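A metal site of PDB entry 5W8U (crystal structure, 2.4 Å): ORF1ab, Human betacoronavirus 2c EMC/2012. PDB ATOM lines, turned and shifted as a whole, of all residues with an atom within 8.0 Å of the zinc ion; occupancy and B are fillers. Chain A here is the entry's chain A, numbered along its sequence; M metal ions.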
ATOM      1  N   TRP A 190      16.415  -2.412 -20.300  1.00  0.00           N
ATOM      2  CA  TRP A 190      17.398  -3.360 -19.787  1.00  0.00           C
ATOM      3  C   TRP A 190      16.881  -4.785 -19.932  1.00  0.00           C
ATOM      4  O   TRP A 190      15.673  -5.034 -19.941  1.00  0.00           O
ATOM      5  CB  TRP A 190      17.775  -3.057 -18.328  1.00  0.00           C
ATOM      6  CG  TRP A 190      16.693  -3.200 -17.300  1.00  0.00           C
ATOM      7  CD1 TRP A 190      16.456  -4.290 -16.503  1.00  0.00           C
ATOM      8  CD2 TRP A 190      15.723  -2.213 -16.918  1.00  0.00           C
ATOM      9  NE1 TRP A 190      15.381  -4.047 -15.664  1.00  0.00           N
ATOM     10  CE2 TRP A 190      14.918  -2.782 -15.900  1.00  0.00           C
ATOM     11  CE3 TRP A 190      15.447  -0.907 -17.353  1.00  0.00           C
ATOM     12  CZ2 TRP A 190      13.869  -2.078 -15.313  1.00  0.00           C
ATOM     13  CZ3 TRP A 190      14.401  -0.224 -16.767  1.00  0.00           C
ATOM     14  CH2 TRP A 190      13.623  -0.813 -15.747  1.00  0.00           C
ATOM     15  N   CYS A 191      17.831  -5.706 -20.063  1.00  0.00           N
ATOM     16  CA  CYS A 191      17.597  -7.136 -20.147  1.00  0.00           C
ATOM     17  C   CYS A 191      18.731  -7.825 -19.403  1.00  0.00           C
ATOM     18  O   CYS A 191      19.900  -7.478 -19.627  1.00  0.00           O
ATOM     19  CB  CYS A 191      17.540  -7.599 -21.610  1.00  0.00           C
ATOM     20  SG  CYS A 191      17.912  -9.333 -21.917  1.00  0.00           S
ATOM     21  N   ASN A 192      18.393  -8.768 -18.522  1.00  0.00           N
ATOM     22  CA  ASN A 192      19.404  -9.350 -17.642  1.00  0.00           C
ATOM     23  C   ASN A 192      20.518 -10.046 -18.410  1.00  0.00           C
ATOM     24  O   ASN A 192      21.601 -10.262 -17.834  1.00  0.00           O
ATOM     25  CB  ASN A 192      18.754 -10.332 -16.668  1.00  0.00           C
ATOM     26  CG  ASN A 192      17.905  -9.633 -15.616  1.00  0.00           C
ATOM     27  OD1 ASN A 192      18.139  -8.471 -15.304  1.00  0.00           O
ATOM     28  ND2 ASN A 192      16.932 -10.355 -15.072  1.00  0.00           N
ATOM     29  N   VAL A 193      20.301 -10.399 -19.665  1.00  0.00           N
ATOM     30  CA  VAL A 193      21.327 -11.031 -20.490  1.00  0.00           C
ATOM     31  C   VAL A 193      21.995 -10.035 -21.417  1.00  0.00           C
ATOM     32  O   VAL A 193      23.216 -10.071 -21.603  1.00  0.00           O
ATOM     33  CB  VAL A 193      20.720 -12.207 -21.278  1.00  0.00           C
ATOM     34  CG1 VAL A 193      21.820 -13.020 -21.961  1.00  0.00           C
ATOM     35  CG2 VAL A 193      19.905 -13.103 -20.357  1.00  0.00           C
ATOM     36  N   CYS A 194      21.212  -9.125 -22.015  1.00  0.00           N
ATOM     37  CA  CYS A 194      21.730  -8.211 -23.027  1.00  0.00           C
ATOM     38  C   CYS A 194      22.349  -6.942 -22.432  1.00  0.00           C
ATOM     39  O   CYS A 194      23.211  -6.342 -23.076  1.00  0.00           O
ATOM     40  CB  CYS A 194      20.610  -7.818 -24.001  1.00  0.00           C
ATOM     41  SG  CYS A 194      19.920  -9.207 -24.905  1.00  0.00           S
ATOM     42  N   GLY A 195      21.927  -6.525 -21.253  1.00  0.00           N
ATOM     43  CA  GLY A 195      22.443  -5.333 -20.621  1.00  0.00           C
ATOM     44  C   GLY A 195      21.426  -4.204 -20.624  1.00  0.00           C
ATOM     45  O   GLY A 195      20.222  -4.404 -20.848  1.00  0.00           O
ATOM     46  N   TYR A 224       8.338  -6.893 -21.926  1.00  0.00           N
ATOM     47  CA  TYR A 224       8.006  -7.470 -23.225  1.00  0.00           C
ATOM     48  C   TYR A 224       9.201  -8.303 -23.669  1.00  0.00           C
ATOM     49  O   TYR A 224      10.295  -8.193 -23.112  1.00  0.00           O
ATOM     50  CB  TYR A 224       7.641  -6.385 -24.246  1.00  0.00           C
ATOM     51  CG  TYR A 224       8.702  -5.314 -24.390  1.00  0.00           C
ATOM     52  CD1 TYR A 224       9.606  -5.327 -25.444  1.00  0.00           C
ATOM     53  CD2 TYR A 224       8.802  -4.284 -23.460  1.00  0.00           C
ATOM     54  CE1 TYR A 224      10.577  -4.353 -25.569  1.00  0.00           C
ATOM     55  CE2 TYR A 224       9.770  -3.302 -23.574  1.00  0.00           C
ATOM     56  CZ  TYR A 224      10.653  -3.339 -24.631  1.00  0.00           C
ATOM     57  OH  TYR A 224      11.617  -2.358 -24.736  1.00  0.00           O
ATOM     58  N   VAL A 225       8.987  -9.132 -24.692  1.00  0.00           N
ATOM     59  CA  VAL A 225      10.006 -10.080 -25.111  1.00  0.00           C
ATOM     60  C   VAL A 225      11.199  -9.344 -25.711  1.00  0.00           C
ATOM     61  O   VAL A 225      11.044  -8.373 -26.470  1.00  0.00           O
ATOM     62  CB  VAL A 225       9.416 -11.112 -26.083  1.00  0.00           C
ATOM     63  CG1 VAL A 225       9.053 -10.489 -27.429  1.00  0.00           C
ATOM     64  CG2 VAL A 225      10.377 -12.291 -26.269  1.00  0.00           C
ATOM     65  N   CYS A 226      12.392  -9.776 -25.337  1.00  0.00           N
ATOM     66  CA  CYS A 226      13.641  -9.252 -25.856  1.00  0.00           C
ATOM     67  C   CYS A 226      14.074 -10.021 -27.100  1.00  0.00           C
ATOM     68  O   CYS A 226      13.609 -11.125 -27.367  1.00  0.00           O
ATOM     69  CB  CYS A 226      14.739  -9.330 -24.782  1.00  0.00           C
ATOM     70  SG  CYS A 226      16.220  -8.409 -25.195  1.00  0.00           S
ATOM     71  N   GLN A 227      14.998  -9.419 -27.859  1.00  0.00           N
ATOM     72  CA  GLN A 227      15.497 -10.078 -29.065  1.00  0.00           C
ATOM     73  C   GLN A 227      16.191 -11.395 -28.735  1.00  0.00           C
ATOM     74  O   GLN A 227      16.237 -12.299 -29.578  1.00  0.00           O
ATOM     75  CB  GLN A 227      16.440  -9.154 -29.838  1.00  0.00           C
ATOM     76  CG  GLN A 227      16.627  -9.552 -31.292  1.00  0.00           C
ATOM     77  CD  GLN A 227      17.525  -8.596 -32.090  1.00  0.00           C
ATOM     78  OE1 GLN A 227      17.504  -7.385 -31.875  1.00  0.00           O
ATOM     79  NE2 GLN A 227      18.307  -9.142 -33.001  1.00  0.00           N
ATOM     80  N   CYS A 228      16.721 -11.535 -27.521  1.00  0.00           N
ATOM     81  CA  CYS A 228      17.339 -12.775 -27.076  1.00  0.00           C
ATOM     82  C   CYS A 228      16.324 -13.823 -26.636  1.00  0.00           C
ATOM     83  O   CYS A 228      16.723 -14.958 -26.332  1.00  0.00           O
ATOM     84  CB  CYS A 228      18.309 -12.502 -25.924  1.00  0.00           C
ATOM     85  SG  CYS A 228      17.516 -12.002 -24.372  1.00  0.00           S
ATOM     86  N   GLY A 229      15.043 -13.484 -26.583  1.00  0.00           N
ATOM     87  CA  GLY A 229      14.036 -14.393 -26.066  1.00  0.00           C
ATOM     88  C   GLY A 229      13.664 -14.187 -24.611  1.00  0.00           C
ATOM     89  O   GLY A 229      12.628 -14.719 -24.178  1.00  0.00           O
ATOM     90  N   GLY A 230      14.465 -13.452 -23.848  1.00  0.00           N
ATOM     91  CA  GLY A 230      14.165 -13.164 -22.459  1.00  0.00           C
ATOM     92  C   GLY A 230      13.131 -12.074 -22.302  1.00  0.00           C
ATOM     93  O   GLY A 230      12.408 -11.712 -23.245  1.00  0.00           O
ATOM     94  N   GLU A 231      13.060 -11.531 -21.103  1.00  0.00           N
ATOM     95  CA  GLU A 231      12.129 -10.451 -20.828  1.00  0.00           C
ATOM     96  C   GLU A 231      12.917  -9.150 -20.724  1.00  0.00           C
ATOM     97  O   GLU A 231      13.895  -9.061 -19.970  1.00  0.00           O
ATOM     98  CB  GLU A 231      11.309 -10.737 -19.569  1.00  0.00           C
ATOM     99  CG  GLU A 231      10.084 -11.579 -19.951  1.00  0.00           C
ATOM    100  CD  GLU A 231       8.931 -11.652 -18.981  1.00  0.00           C
ATOM    101  OE1 GLU A 231       7.778 -11.888 -19.446  1.00  0.00           O
ATOM    102  OE2 GLU A 231       9.178 -11.474 -17.749  1.00  0.00           O
ATOM    103  N   ARG A 232      12.527  -8.183 -21.528  1.00  0.00           N
ATOM    104  CA  ARG A 232      13.134  -6.868 -21.552  1.00  0.00           C
ATOM    105  C   ARG A 232      12.228  -5.890 -20.819  1.00  0.00           C
ATOM    106  O   ARG A 232      11.000  -6.024 -20.830  1.00  0.00           O
ATOM    107  CB  ARG A 232      13.367  -6.410 -22.985  1.00  0.00           C
ATOM    108  CG  ARG A 232      14.088  -5.074 -23.092  1.00  0.00           C
ATOM    109  CD  ARG A 232      14.715  -4.901 -24.475  1.00  0.00           C
ATOM    110  NE  ARG A 232      13.746  -5.169 -25.533  1.00  0.00           N
ATOM    111  CZ  ARG A 232      14.036  -5.209 -26.832  1.00  0.00           C
ATOM    112  NH1 ARG A 232      15.292  -4.999 -27.240  1.00  0.00           N
ATOM    113  NH2 ARG A 232      13.087  -5.453 -27.725  1.00  0.00           N
ATOM    114  N   HIS A 233      12.841  -4.916 -20.165  1.00  0.00           N
ATOM    115  CA  HIS A 233      12.125  -3.898 -19.434  1.00  0.00           C
ATOM    116  C   HIS A 233      12.441  -2.526 -20.006  1.00  0.00           C
ATOM    117  O   HIS A 233      13.505  -2.306 -20.594  1.00  0.00           O
ATOM    118  CB  HIS A 233      12.465  -3.948 -17.950  1.00  0.00           C
ATOM    119  CG  HIS A 233      12.337  -5.315 -17.361  1.00  0.00           C
ATOM    120  ND1 HIS A 233      11.145  -5.822 -16.888  1.00  0.00           N
ATOM    121  CD2 HIS A 233      13.256  -6.299 -17.192  1.00  0.00           C
ATOM    122  CE1 HIS A 233      11.335  -7.053 -16.437  1.00  0.00           C
ATOM    123  NE2 HIS A 233      12.607  -7.368 -16.610  1.00  0.00           N
HETATM  124 ZN    ZN M   1      17.805  -9.756 -24.092  1.00  0.00          ZN
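Within 4 Å of the zinc ion: Cys 191, Cys 194, Cys 226 and Cys 228.
The zinc ion is bound by SG of Cys 191 (2.2 Å), SG of Cys 228 (2.3 Å), SG of Cys 194 (2.3 Å) and SG of Cys 226 (2.4 Å).
The side-chain sulfur (SG) of Cys 191 sits close to the backbone NH (N) of Val 193 (3.5 Å). The backbone NH (N) of Gly 230 lies close to the side-chain sulfur (SG) of Cys 228 (3.4 Å).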
